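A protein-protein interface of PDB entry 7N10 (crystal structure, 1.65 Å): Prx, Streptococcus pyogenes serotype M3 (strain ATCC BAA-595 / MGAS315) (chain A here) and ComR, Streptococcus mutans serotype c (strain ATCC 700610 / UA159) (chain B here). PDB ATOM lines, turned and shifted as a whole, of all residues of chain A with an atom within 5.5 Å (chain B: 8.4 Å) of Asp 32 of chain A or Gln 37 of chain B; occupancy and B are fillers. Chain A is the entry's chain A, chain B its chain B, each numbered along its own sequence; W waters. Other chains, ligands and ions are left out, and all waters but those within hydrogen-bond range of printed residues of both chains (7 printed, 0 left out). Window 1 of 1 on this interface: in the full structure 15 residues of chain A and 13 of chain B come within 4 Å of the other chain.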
ATOM      1  N   MET A   1       3.077   1.970 -26.740  1.00  0.00           N
ATOM      2  CA  MET A   1       3.515   3.393 -26.747  1.00  0.00           C
ATOM      3  C   MET A   1       4.318   3.704 -25.495  1.00  0.00           C
ATOM      4  O   MET A   1       3.958   3.287 -24.393  1.00  0.00           O
ATOM      5  CB  MET A   1       2.314   4.333 -26.838  1.00  0.00           C
ATOM      6  CG  MET A   1       2.651   5.793 -26.547  1.00  0.00           C
ATOM      7  SD  MET A   1       1.374   6.935 -27.129  1.00  0.00           S
ATOM      8  CE  MET A   1       0.024   6.488 -26.045  1.00  0.00           C
ATOM      9  N   LEU A   2       5.419   4.427 -25.676  1.00  0.00           N
ATOM     10  CA  LEU A   2       6.286   4.841 -24.587  1.00  0.00           C
ATOM     11  C   LEU A   2       6.363   6.361 -24.579  1.00  0.00           C
ATOM     12  O   LEU A   2       6.842   6.965 -25.546  1.00  0.00           O
ATOM     13  CB  LEU A   2       7.676   4.215 -24.746  1.00  0.00           C
ATOM     14  CG  LEU A   2       8.728   4.614 -23.713  1.00  0.00           C
ATOM     15  CD1 LEU A   2       8.235   4.339 -22.297  1.00  0.00           C
ATOM     16  CD2 LEU A   2      10.026   3.873 -23.993  1.00  0.00           C
ATOM     17  N   GLU A   6       7.460   8.634 -19.164  1.00  0.00           N
ATOM     18  CA  GLU A   6       7.542   7.295 -18.581  1.00  0.00           C
ATOM     19  C   GLU A   6       8.984   6.798 -18.560  1.00  0.00           C
ATOM     20  O   GLU A   6       9.451   6.226 -17.564  1.00  0.00           O
ATOM     21  CB  GLU A   6       6.665   6.321 -19.369  1.00  0.00           C
ATOM     22  CG  GLU A   6       5.174   6.529 -19.202  1.00  0.00           C
ATOM     23  CD  GLU A   6       4.349   5.742 -20.209  1.00  0.00           C
ATOM     24  OE1 GLU A   6       4.874   5.407 -21.294  1.00  0.00           O
ATOM     25  OE2 GLU A   6       3.164   5.461 -19.922  1.00  0.00           O
ATOM     26  N   ALA A  22      16.923  -2.295 -23.090  1.00  0.00           N
ATOM     27  CA  ALA A  22      16.198  -3.141 -24.026  1.00  0.00           C
ATOM     28  C   ALA A  22      14.870  -2.487 -24.396  1.00  0.00           C
ATOM     29  O   ALA A  22      14.129  -2.027 -23.522  1.00  0.00           O
ATOM     30  CB  ALA A  22      15.970  -4.526 -23.420  1.00  0.00           C
ATOM     31  N   ILE A  23      14.572  -2.477 -25.695  1.00  0.00           N
ATOM     32  CA  ILE A  23      13.449  -1.758 -26.288  1.00  0.00           C
ATOM     33  C   ILE A  23      12.644  -2.722 -27.142  1.00  0.00           C
ATOM     34  O   ILE A  23      13.212  -3.514 -27.904  1.00  0.00           O
ATOM     35  CB  ILE A  23      13.939  -0.582 -27.164  1.00  0.00           C
ATOM     36  CG1 ILE A  23      14.576   0.518 -26.312  1.00  0.00           C
ATOM     37  CG2 ILE A  23      12.812  -0.042 -28.041  1.00  0.00           C
ATOM     38  CD1 ILE A  23      13.633   1.237 -25.403  1.00  0.00           C
ATOM     39  N   VAL A  24      11.319  -2.623 -27.053  1.00  0.00           N
ATOM     40  CA  VAL A  24      10.401  -3.324 -27.939  1.00  0.00           C
ATOM     41  C   VAL A  24       9.824  -2.308 -28.912  1.00  0.00           C
ATOM     42  O   VAL A  24       9.310  -1.257 -28.495  1.00  0.00           O
ATOM     43  CB  VAL A  24       9.269  -4.021 -27.164  1.00  0.00           C
ATOM     44  CG1 VAL A  24       8.242  -4.607 -28.128  1.00  0.00           C
ATOM     45  CG2 VAL A  24       9.820  -5.107 -26.281  1.00  0.00           C
ATOM     46  N   ARG A  25       9.888  -2.637 -30.197  1.00  0.00           N
ATOM     47  CA  ARG A  25       9.319  -1.824 -31.261  1.00  0.00           C
ATOM     48  C   ARG A  25       8.185  -2.592 -31.924  1.00  0.00           C
ATOM     49  O   ARG A  25       8.256  -3.817 -32.071  1.00  0.00           O
ATOM     50  CB  ARG A  25      10.384  -1.451 -32.294  1.00  0.00           C
ATOM     51  CG  ARG A  25      11.408  -0.464 -31.756  1.00  0.00           C
ATOM     52  CD  ARG A  25      12.552  -0.233 -32.729  1.00  0.00           C
ATOM     53  NE  ARG A  25      13.471   0.771 -32.214  1.00  0.00           N
ATOM     54  CZ  ARG A  25      13.371   2.071 -32.459  1.00  0.00           C
ATOM     55  NH1 ARG A  25      12.440   2.552 -33.266  1.00  0.00           N
ATOM     56  NH2 ARG A  25      14.225   2.908 -31.880  1.00  0.00           N
ATOM     57  N   ILE A  30       8.877   2.836 -31.383  1.00  0.00           N
ATOM     58  CA  ILE A  30       9.167   2.389 -30.027  1.00  0.00           C
ATOM     59  C   ILE A  30       7.847   2.141 -29.310  1.00  0.00           C
ATOM     60  O   ILE A  30       6.970   3.012 -29.272  1.00  0.00           O
ATOM     61  CB  ILE A  30      10.030   3.420 -29.287  1.00  0.00           C
ATOM     62  CG1 ILE A  30      11.395   3.565 -29.962  1.00  0.00           C
ATOM     63  CG2 ILE A  30      10.209   3.006 -27.823  1.00  0.00           C
ATOM     64  CD1 ILE A  30      12.276   4.658 -29.359  1.00  0.00           C
ATOM     65  N   PHE A  31       7.695   0.945 -28.744  1.00  0.00           N
ATOM     66  CA  PHE A  31       6.466   0.540 -28.070  1.00  0.00           C
ATOM     67  C   PHE A  31       6.616   0.409 -26.567  1.00  0.00           C
ATOM     68  O   PHE A  31       5.674   0.723 -25.833  1.00  0.00           O
ATOM     69  CB  PHE A  31       5.979  -0.800 -28.640  1.00  0.00           C
ATOM     70  CG  PHE A  31       4.856  -1.424 -27.870  1.00  0.00           C
ATOM     71  CD1 PHE A  31       3.551  -0.972 -28.019  1.00  0.00           C
ATOM     72  CD2 PHE A  31       5.095  -2.481 -27.009  1.00  0.00           C
ATOM     73  CE1 PHE A  31       2.507  -1.558 -27.298  1.00  0.00           C
ATOM     74  CE2 PHE A  31       4.062  -3.072 -26.297  1.00  0.00           C
ATOM     75  CZ  PHE A  31       2.766  -2.607 -26.443  1.00  0.00           C
ATOM     76  N   ASP A  32       7.774  -0.058 -26.093  1.00  0.00           N
ATOM     77  CA  ASP A  32       7.953  -0.321 -24.667  1.00  0.00           C
ATOM     78  C   ASP A  32       9.442  -0.453 -24.394  1.00  0.00           C
ATOM     79  O   ASP A  32      10.238  -0.605 -25.319  1.00  0.00           O
ATOM     80  CB  ASP A  32       7.228  -1.603 -24.251  1.00  0.00           C
ATOM     81  CG  ASP A  32       6.958  -1.697 -22.752  1.00  0.00           C
ATOM     82  OD1 ASP A  32       7.294  -0.772 -21.967  1.00  0.00           O
ATOM     83  OD2 ASP A  32       6.426  -2.755 -22.349  1.00  0.00           O
ATOM     84  N   TYR A  33       9.807  -0.411 -23.113  1.00  0.00           N
ATOM     85  CA  TYR A  33      11.115  -0.877 -22.662  1.00  0.00           C
ATOM     86  C   TYR A  33      10.954  -2.188 -21.893  1.00  0.00           C
ATOM     87  O   TYR A  33       9.855  -2.592 -21.524  1.00  0.00           O
ATOM     88  CB  TYR A  33      11.822   0.181 -21.800  1.00  0.00           C
ATOM     89  CG  TYR A  33      11.093   0.609 -20.548  1.00  0.00           C
ATOM     90  CD1 TYR A  33      11.279  -0.054 -19.333  1.00  0.00           C
ATOM     91  CD2 TYR A  33      10.234   1.700 -20.569  1.00  0.00           C
ATOM     92  CE1 TYR A  33      10.613   0.351 -18.186  1.00  0.00           C
ATOM     93  CE2 TYR A  33       9.567   2.111 -19.426  1.00  0.00           C
ATOM     94  CZ  TYR A  33       9.754   1.438 -18.243  1.00  0.00           C
ATOM     95  OH  TYR A  33       9.092   1.848 -17.114  1.00  0.00           O
ATOM     96  N   VAL A  34      12.080  -2.868 -21.663  1.00  0.00           N
ATOM     97  CA  VAL A  34      12.094  -4.130 -20.925  1.00  0.00           C
ATOM     98  C   VAL A  34      13.205  -4.074 -19.885  1.00  0.00           C
ATOM     99  O   VAL A  34      14.389  -3.987 -20.240  1.00  0.00           O
ATOM    100  CB  VAL A  34      12.311  -5.348 -21.839  1.00  0.00           C
ATOM    101  CG1 VAL A  34      12.171  -6.638 -21.034  1.00  0.00           C
ATOM    102  CG2 VAL A  34      11.350  -5.341 -23.011  1.00  0.00           C
ATOM    103  N   ILE B  12      -7.304   0.225  -9.975  1.00  0.00           N
ATOM    104  CA  ILE B  12      -7.515  -0.585 -11.168  1.00  0.00           C
ATOM    105  C   ILE B  12      -7.212  -2.043 -10.874  1.00  0.00           C
ATOM    106  O   ILE B  12      -7.840  -2.937 -11.448  1.00  0.00           O
ATOM    107  CB  ILE B  12      -6.710  -0.094 -12.386  1.00  0.00           C
ATOM    108  CG1 ILE B  12      -5.206  -0.299 -12.192  1.00  0.00           C
ATOM    109  CG2 ILE B  12      -7.050   1.352 -12.706  1.00  0.00           C
ATOM    110  CD1 ILE B  12      -4.397   0.129 -13.387  1.00  0.00           C
ATOM    111  N   LYS B  23      -4.236  -9.540 -15.993  1.00  0.00           N
ATOM    112  CA  LYS B  23      -3.642  -8.373 -16.642  1.00  0.00           C
ATOM    113  C   LYS B  23      -3.617  -8.554 -18.154  1.00  0.00           C
ATOM    114  O   LYS B  23      -3.860  -7.605 -18.918  1.00  0.00           O
ATOM    115  CB  LYS B  23      -2.237  -8.138 -16.090  1.00  0.00           C
ATOM    116  CG  LYS B  23      -2.247  -7.565 -14.681  1.00  0.00           C
ATOM    117  CD  LYS B  23      -0.840  -7.230 -14.195  1.00  0.00           C
ATOM    118  CE  LYS B  23      -0.052  -8.485 -13.867  1.00  0.00           C
ATOM    119  NZ  LYS B  23      -0.455  -9.074 -12.566  1.00  0.00           N
ATOM    120  N   CYS B  27      -5.140  -6.185 -21.240  1.00  0.00           N
ATOM    121  CA  CYS B  27      -4.318  -5.644 -22.321  1.00  0.00           C
ATOM    122  C   CYS B  27      -4.717  -6.124 -23.716  1.00  0.00           C
ATOM    123  O   CYS B  27      -4.223  -5.560 -24.698  1.00  0.00           O
ATOM    124  CB  CYS B  27      -2.845  -5.977 -22.065  1.00  0.00           C
ATOM    125  SG  CYS B  27      -2.174  -5.174 -20.583  1.00  0.00           S
ATOM    126  N   GLU B  30      -2.512  -6.205 -26.859  1.00  0.00           N
ATOM    127  CA  GLU B  30      -1.321  -5.469 -26.448  1.00  0.00           C
ATOM    128  C   GLU B  30      -0.891  -4.463 -27.507  1.00  0.00           C
ATOM    129  O   GLU B  30       0.287  -4.119 -27.619  1.00  0.00           O
ATOM    130  CB  GLU B  30      -0.179  -6.431 -26.096  1.00  0.00           C
ATOM    131  CG  GLU B  30      -0.474  -7.267 -24.843  1.00  0.00           C
ATOM    132  CD  GLU B  30       0.728  -8.031 -24.311  1.00  0.00           C
ATOM    133  OE1 GLU B  30       1.730  -7.389 -23.919  1.00  0.00           O
ATOM    134  OE2 GLU B  30       0.659  -9.280 -24.267  1.00  0.00           O
ATOM    135  N   SER B  31      -1.845  -3.962 -28.293  1.00  0.00           N
ATOM    136  CA  SER B  31      -1.516  -2.906 -29.242  1.00  0.00           C
ATOM    137  C   SER B  31      -1.447  -1.541 -28.571  1.00  0.00           C
ATOM    138  O   SER B  31      -0.714  -0.663 -29.045  1.00  0.00           O
ATOM    139  CB  SER B  31      -2.546  -2.879 -30.374  1.00  0.00           C
ATOM    140  OG  SER B  31      -3.803  -2.460 -29.875  1.00  0.00           O
ATOM    141  N   GLN B  32      -2.182  -1.355 -27.467  1.00  0.00           N
ATOM    142  CA  GLN B  32      -2.212  -0.096 -26.735  1.00  0.00           C
ATOM    143  C   GLN B  32      -1.495  -0.162 -25.392  1.00  0.00           C
ATOM    144  O   GLN B  32      -1.170   0.888 -24.827  1.00  0.00           O
ATOM    145  CB  GLN B  32      -3.657   0.339 -26.455  1.00  0.00           C
ATOM    146  CG  GLN B  32      -4.547   0.575 -27.666  1.00  0.00           C
ATOM    147  CD  GLN B  32      -3.960   1.546 -28.660  1.00  0.00           C
ATOM    148  OE1 GLN B  32      -3.803   2.732 -28.367  1.00  0.00           O
ATOM    149  NE2 GLN B  32      -3.664   1.058 -29.858  1.00  0.00           N
ATOM    150  N   LEU B  33      -1.277  -1.359 -24.856  1.00  0.00           N
ATOM    151  CA  LEU B  33      -0.799  -1.520 -23.485  1.00  0.00           C
ATOM    152  C   LEU B  33      -0.153  -2.886 -23.368  1.00  0.00           C
ATOM    153  O   LEU B  33      -0.812  -3.900 -23.622  1.00  0.00           O
ATOM    154  CB  LEU B  33      -1.957  -1.387 -22.495  1.00  0.00           C
ATOM    155  CG  LEU B  33      -1.632  -1.424 -21.008  1.00  0.00           C
ATOM    156  CD1 LEU B  33      -0.844  -0.187 -20.617  1.00  0.00           C
ATOM    157  CD2 LEU B  33      -2.894  -1.537 -20.162  1.00  0.00           C
ATOM    158  N   SER B  34       1.118  -2.924 -22.975  1.00  0.00           N
ATOM    159  CA  SER B  34       1.755  -4.199 -22.701  1.00  0.00           C
ATOM    160  C   SER B  34       1.423  -4.652 -21.283  1.00  0.00           C
ATOM    161  O   SER B  34       1.119  -3.851 -20.399  1.00  0.00           O
ATOM    162  CB  SER B  34       3.268  -4.098 -22.867  1.00  0.00           C
ATOM    163  OG  SER B  34       3.840  -3.463 -21.725  1.00  0.00           O
ATOM    164  N   THR B  35       1.492  -5.969 -21.071  1.00  0.00           N
ATOM    165  CA  THR B  35       1.319  -6.509 -19.728  1.00  0.00           C
ATOM    166  C   THR B  35       2.344  -5.913 -18.765  1.00  0.00           C
ATOM    167  O   THR B  35       2.033  -5.653 -17.595  1.00  0.00           O
ATOM    168  CB  THR B  35       1.426  -8.033 -19.774  1.00  0.00           C
ATOM    169  OG1 THR B  35       0.342  -8.553 -20.571  1.00  0.00           O
ATOM    170  CG2 THR B  35       1.326  -8.617 -18.381  1.00  0.00           C
ATOM    171  N   ARG B  36       3.567  -5.667 -19.245  1.00  0.00           N
ATOM    172  CA  ARG B  36       4.578  -5.032 -18.402  1.00  0.00           C
ATOM    173  C   ARG B  36       4.121  -3.654 -17.940  1.00  0.00           C
ATOM    174  O   ARG B  36       4.266  -3.302 -16.762  1.00  0.00           O
ATOM    175  CB  ARG B  36       5.911  -4.909 -19.153  1.00  0.00           C
ATOM    176  CG  ARG B  36       6.643  -6.225 -19.373  1.00  0.00           C
ATOM    177  CD  ARG B  36       7.898  -6.032 -20.210  1.00  0.00           C
ATOM    178  NE  ARG B  36       7.604  -5.402 -21.489  1.00  0.00           N
ATOM    179  CZ  ARG B  36       7.243  -6.056 -22.581  1.00  0.00           C
ATOM    180  NH1 ARG B  36       7.303  -7.380 -22.648  1.00  0.00           N
ATOM    181  NH2 ARG B  36       6.817  -5.370 -23.642  1.00  0.00           N
ATOM    182  N   GLN B  37       3.609  -2.841 -18.871  1.00  0.00           N
ATOM    183  CA  GLN B  37       3.179  -1.485 -18.530  1.00  0.00           C
ATOM    184  C   GLN B  37       2.032  -1.492 -17.523  1.00  0.00           C
ATOM    185  O   GLN B  37       2.003  -0.679 -16.590  1.00  0.00           O
ATOM    186  CB  GLN B  37       2.779  -0.745 -19.808  1.00  0.00           C
ATOM    187  CG  GLN B  37       3.993  -0.359 -20.675  1.00  0.00           C
ATOM    188  CD  GLN B  37       3.642   0.003 -22.107  1.00  0.00           C
ATOM    189  OE1 GLN B  37       2.607  -0.413 -22.651  1.00  0.00           O
ATOM    190  NE2 GLN B  37       4.510   0.782 -22.734  1.00  0.00           N
ATOM    191  N   LEU B  38       1.059  -2.387 -17.705  1.00  0.00           N
ATOM    192  CA  LEU B  38      -0.013  -2.493 -16.717  1.00  0.00           C
ATOM    193  C   LEU B  38       0.539  -2.897 -15.354  1.00  0.00           C
ATOM    194  O   LEU B  38       0.132  -2.344 -14.326  1.00  0.00           O
ATOM    195  CB  LEU B  38      -1.066  -3.498 -17.182  1.00  0.00           C
ATOM    196  CG  LEU B  38      -2.266  -3.668 -16.255  1.00  0.00           C
ATOM    197  CD1 LEU B  38      -2.929  -2.337 -15.927  1.00  0.00           C
ATOM    198  CD2 LEU B  38      -3.266  -4.627 -16.889  1.00  0.00           C
ATOM    199  N   THR B  39       1.471  -3.859 -15.331  1.00  0.00           N
ATOM    200  CA  THR B  39       2.070  -4.285 -14.072  1.00  0.00           C
ATOM    201  C   THR B  39       2.744  -3.113 -13.372  1.00  0.00           C
ATOM    202  O   THR B  39       2.571  -2.915 -12.165  1.00  0.00           O
ATOM    203  CB  THR B  39       3.071  -5.414 -14.326  1.00  0.00           C
ATOM    204  OG1 THR B  39       2.402  -6.533 -14.921  1.00  0.00           O
ATOM    205  CG2 THR B  39       3.733  -5.859 -13.036  1.00  0.00           C
ATOM    206  N   ARG B  40       3.521  -2.327 -14.123  1.00  0.00           N
ATOM    207  CA  ARG B  40       4.196  -1.175 -13.536  1.00  0.00           C
ATOM    208  C   ARG B  40       3.193  -0.178 -12.971  1.00  0.00           C
ATOM    209  O   ARG B  40       3.424   0.418 -11.911  1.00  0.00           O
ATOM    210  CB  ARG B  40       5.076  -0.494 -14.577  1.00  0.00           C
ATOM    211  CG  ARG B  40       6.187  -1.358 -15.106  1.00  0.00           C
ATOM    212  CD  ARG B  40       6.877  -0.650 -16.253  1.00  0.00           C
ATOM    213  NE  ARG B  40       7.630  -1.574 -17.088  1.00  0.00           N
ATOM    214  CZ  ARG B  40       7.725  -1.487 -18.408  1.00  0.00           C
ATOM    215  NH1 ARG B  40       7.113  -0.525 -19.087  1.00  0.00           N
ATOM    216  NH2 ARG B  40       8.434  -2.400 -19.067  1.00  0.00           N
ATOM    217  N   ILE B  41       2.071   0.023 -13.659  1.00  0.00           N
ATOM    218  CA  ILE B  41       1.091   0.971 -13.132  1.00  0.00           C
ATOM    219  C   ILE B  41       0.454   0.435 -11.848  1.00  0.00           C
ATOM    220  O   ILE B  41       0.306   1.169 -10.861  1.00  0.00           O
ATOM    221  CB  ILE B  41       0.037   1.305 -14.201  1.00  0.00           C
ATOM    222  CG1 ILE B  41       0.642   2.173 -15.300  1.00  0.00           C
ATOM    223  CG2 ILE B  41      -1.145   2.018 -13.554  1.00  0.00           C
ATOM    224  CD1 ILE B  41      -0.180   2.234 -16.585  1.00  0.00           C
ATOM    225  N   GLU B  42       0.086  -0.853 -11.829  1.00  0.00           N
ATOM    226  CA  GLU B  42      -0.616  -1.410 -10.678  1.00  0.00           C
ATOM    227  C   GLU B  42       0.242  -1.348  -9.420  1.00  0.00           C
ATOM    228  O   GLU B  42      -0.275  -1.101  -8.321  1.00  0.00           O
ATOM    229  CB  GLU B  42      -1.042  -2.852 -10.967  1.00  0.00           C
ATOM    230  CG  GLU B  42      -2.253  -2.923 -11.884  1.00  0.00           C
ATOM    231  CD  GLU B  42      -2.909  -4.289 -11.956  1.00  0.00           C
ATOM    232  OE1 GLU B  42      -2.417  -5.245 -11.317  1.00  0.00           O
ATOM    233  OE2 GLU B  42      -3.947  -4.395 -12.646  1.00  0.00           O
ATOM    234  N   SER B  43       1.545  -1.560  -9.560  1.00  0.00           N
ATOM    235  CA  SER B  43       2.456  -1.563  -8.424  1.00  0.00           C
ATOM    236  C   SER B  43       2.969  -0.176  -8.066  1.00  0.00           C
ATOM    237  O   SER B  43       3.736  -0.047  -7.102  1.00  0.00           O
ATOM    238  CB  SER B  43       3.650  -2.474  -8.706  1.00  0.00           C
ATOM    239  OG  SER B  43       4.423  -1.963  -9.778  1.00  0.00           O
ATOM    240  N   GLY B  44       2.580   0.855  -8.808  1.00  0.00           N
ATOM    241  CA  GLY B  44       3.108   2.185  -8.591  1.00  0.00           C
ATOM    242  C   GLY B  44       4.492   2.424  -9.152  1.00  0.00           C
ATOM    243  O   GLY B  44       5.030   3.525  -8.979  1.00  0.00           O
ATOM    244  N   GLN B  45       5.088   1.429  -9.818  1.00  0.00           N
ATOM    245  CA  GLN B  45       6.399   1.624 -10.428  1.00  0.00           C
ATOM    246  C   GLN B  45       6.360   2.746 -11.456  1.00  0.00           C
ATOM    247  O   GLN B  45       7.265   3.587 -11.511  1.00  0.00           O
ATOM    248  CB  GLN B  45       6.868   0.322 -11.079  1.00  0.00           C
ATOM    249  CG  GLN B  45       8.366   0.105 -11.047  1.00  0.00           C
ATOM    250  CD  GLN B  45       8.815  -1.091 -11.876  1.00  0.00           C
ATOM    251  OE1 GLN B  45       9.408  -0.940 -12.953  1.00  0.00           O
ATOM    252  NE2 GLN B  45       8.558  -2.286 -11.364  1.00  0.00           N
ATOM    253  N   SER B  46       5.314   2.778 -12.279  1.00  0.00           N
ATOM    254  CA  SER B  46       5.160   3.781 -13.322  1.00  0.00           C
ATOM    255  C   SER B  46       3.905   4.599 -13.062  1.00  0.00           C
ATOM    256  O   SER B  46       2.840   4.040 -12.769  1.00  0.00           O
ATOM    257  CB  SER B  46       5.074   3.137 -14.713  1.00  0.00           C
ATOM    258  OG  SER B  46       6.335   2.629 -15.089  1.00  0.00           O
ATOM    259  N   THR B  47       4.043   5.909 -13.164  1.00  0.00           N
ATOM    260  CA  THR B  47       2.900   6.799 -13.075  1.00  0.00           C
ATOM    261  C   THR B  47       2.040   6.596 -14.317  1.00  0.00           C
ATOM    262  O   THR B  47       2.573   6.535 -15.437  1.00  0.00           O
ATOM    263  CB  THR B  47       3.372   8.250 -12.963  1.00  0.00           C
ATOM    264  OG1 THR B  47       4.118   8.418 -11.745  1.00  0.00           O
ATOM    265  CG2 THR B  47       2.182   9.210 -12.950  1.00  0.00           C
ATOM    266  N   PRO B  48       0.725   6.469 -14.172  1.00  0.00           N
ATOM    267  CA  PRO B  48      -0.117   6.304 -15.360  1.00  0.00           C
ATOM    268  C   PRO B  48      -0.121   7.569 -16.199  1.00  0.00           C
ATOM    269  O   PRO B  48      -0.193   8.683 -15.679  1.00  0.00           O
ATOM    270  CB  PRO B  48      -1.510   6.013 -14.785  1.00  0.00           C
ATOM    271  CG  PRO B  48      -1.482   6.572 -13.404  1.00  0.00           C
ATOM    272  CD  PRO B  48      -0.058   6.496 -12.922  1.00  0.00           C
ATOM    273  N   THR B  49      -0.023   7.384 -17.503  1.00  0.00           N
ATOM    274  CA  THR B  49      -0.214   8.449 -18.473  1.00  0.00           C
ATOM    275  C   THR B  49      -1.661   8.438 -18.954  1.00  0.00           C
ATOM    276  O   THR B  49      -2.397   7.468 -18.758  1.00  0.00           O
ATOM    277  CB  THR B  49       0.751   8.273 -19.639  1.00  0.00           C
ATOM    278  OG1 THR B  49       0.537   6.989 -20.234  1.00  0.00           O
ATOM    279  CG2 THR B  49       2.198   8.384 -19.152  1.00  0.00           C
ATOM    280  N   LYS B  52      -2.966   5.611 -21.409  1.00  0.00           N
ATOM    281  CA  LYS B  52      -3.064   4.314 -20.751  1.00  0.00           C
ATOM    282  C   LYS B  52      -4.201   4.301 -19.734  1.00  0.00           C
ATOM    283  O   LYS B  52      -4.934   3.310 -19.626  1.00  0.00           O
ATOM    284  CB  LYS B  52      -1.737   3.964 -20.077  1.00  0.00           C
ATOM    285  CG  LYS B  52      -0.577   3.704 -21.049  1.00  0.00           C
ATOM    286  CD  LYS B  52       0.680   3.242 -20.307  1.00  0.00           C
ATOM    287  CE  LYS B  52       1.764   2.768 -21.269  1.00  0.00           C
ATOM    288  NZ  LYS B  52       2.231   3.861 -22.185  1.00  0.00           N
ATOM    289  N   ILE B  56      -7.380   1.797 -19.942  1.00  0.00           N
ATOM    290  CA  ILE B  56      -7.647   0.852 -18.863  1.00  0.00           C
ATOM    291  C   ILE B  56      -9.055   1.048 -18.318  1.00  0.00           C
ATOM    292  O   ILE B  56      -9.793   0.080 -18.077  1.00  0.00           O
ATOM    293  CB  ILE B  56      -6.602   1.011 -17.746  1.00  0.00           C
ATOM    294  CG1 ILE B  56      -5.227   0.607 -18.261  1.00  0.00           C
ATOM    295  CG2 ILE B  56      -6.982   0.176 -16.521  1.00  0.00           C
ATOM    296  CD1 ILE B  56      -4.083   1.119 -17.406  1.00  0.00           C
HETATM  297  O   HOH W   1       1.031   1.596 -28.557  1.00  0.00           O
HETATM  298  O   HOH W   2       1.444   1.447 -24.324  1.00  0.00           O
HETATM  299  O   HOH W   3       9.885   1.256 -14.722  1.00  0.00           O
HETATM  300  O   HOH W   4       7.969   4.890 -15.568  1.00  0.00           O
HETATM  301  O   HOH W   5       5.974   2.071 -18.085  1.00  0.00           O
HETATM  302  O   HOH W   6       2.324   4.616 -17.426  1.00  0.00           O
HETATM  303  O   HOH W   7       5.804   2.711 -20.834  1.00  0.00           O
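Among the printed residues, merely in contact across the chains: Phe 31 of chain A with Glu 30 of chain B, Phe 31 of chain A with Ser 31 of chain B, Phe 31 of chain A with Ser 34 of chain B, Tyr 33 of chain A with Arg 36 of chain B and Tyr 33 of chain A with Ser 46 of chain B.
Asp 32 of chain A touches just these residues of chain B: Ser 34, Arg 36, Gln 37 and Arg 40. Gln 37 of chain B touches just these residues of chain A: Met 1, Phe 31 and Asp 32. Printed residues of chain A within 4 Å of Ser 46 of chain B: Tyr 33. Of the printed residues of chain A, Arg 40 of chain B touches Asp 32 and Tyr 33. Of the printed residues of chain B, Met 1 of chain A touches Gln 37 and Lys 52. Of the printed residues of chain B, Tyr 33 of chain A touches Arg 36, Arg 40 and Ser 46. Printed residues of chain A within 4 Å of Ser 31 of chain B: Phe 31.
NE2 of Gln 37 of chain B is in hydrogen-bond range of O of Met 1 of chain A (3.1 Å). The backbone carbonyl oxygen (O) of Met 1 of chain A sits at hydrogen-bond distance from the side-chain amino group (NZ) of Lys 52 of chain B (2.9 Å). OG1 of Thr 49 of chain B is in hydrogen-bond range of OE2 of Glu 6 of chain A (3.1 Å). The side-chain carboxylate (OE2) of Glu 6 of chain A lies within salt-bridge range of the side-chain amino group (NZ) of Lys 52 of chain B (2.9 Å). The side-chain amide nitrogen (NE2) of Gln 37 of chain B lies within hydrogen-bond range of the backbone carbonyl oxygen (O) of Phe 31 of chain A, 3.3 Å away. The side-chain carboxylate (OD2) of Asp 32 of chain A sits at hydrogen-bond distance from the side-chain hydroxyl (OG) of Ser 34 of chain B, at 2.8 Å. The side-chain carboxylate of Asp 32 of chain A lies within salt-bridge range of the guanidinium group of Arg 36 of chain B, 2.9 Å away. The side-chain carboxylate (OD1) of Asp 32 of chain A is in hydrogen-bond range of the side-chain amide nitrogen (NE2) of Gln 37 of chain B. The side-chain carboxylate (OD1) of Asp 32 of chain A is in salt-bridge range of the guanidinium group (NH1) of Arg 40 of chain B, at 2.9 Å. The guanidinium group of Arg 40 of chain B is in hydrogen-bond range of the backbone carbonyl oxygen of Tyr 33 of chain A, at 2.8 Å.
The backbone NH of Phe 31 of chain A lies within hydrogen-bond range of the backbone carbonyl oxygen of Val 24 of chain A. The side-chain hydroxyl (OG) of Ser 34 of chain B lies within hydrogen-bond range of the backbone NH (N) of Gln 37 of chain B, at 2.9 Å. O of Arg 40 of chain B is in hydrogen-bond range of OG of Ser 43 of chain B (3.3 Å).
Of the 12 printed residues of chain A, 5 touch a printed residue of chain B. Printed residues of chain A that touch a printed residue of chain B: Met 1, Glu 6, Phe 31, Asp 32 and Tyr 33. Among the printed residues, 15 pairs touch across the chains. Among the printed residues, Asp or Glu carboxylates within 4 Å of a Lys or Arg side-chain nitrogen of the other chain: Glu 6 of chain A with Lys 52 of chain B (2.9 Å), Asp 32 of chain A with Arg 36 of chain B (2.9 Å) and Asp 32 of chain A with Arg 40 of chain B (2.9 Å).
Water W2 lies within hydrogen-bond range of O of Gln 32 of chain B (2.7 Å), OE1 of Gln 37 of chain B (2.8 Å), N of Met 1 of chain A (3.0 Å) and NZ of Lys 52 of chain B (3.3 Å). Water W4 lies within hydrogen-bond range of O of Glu 6 of chain A (2.8 Å) and OG of Ser 46 of chain B (2.8 Å).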
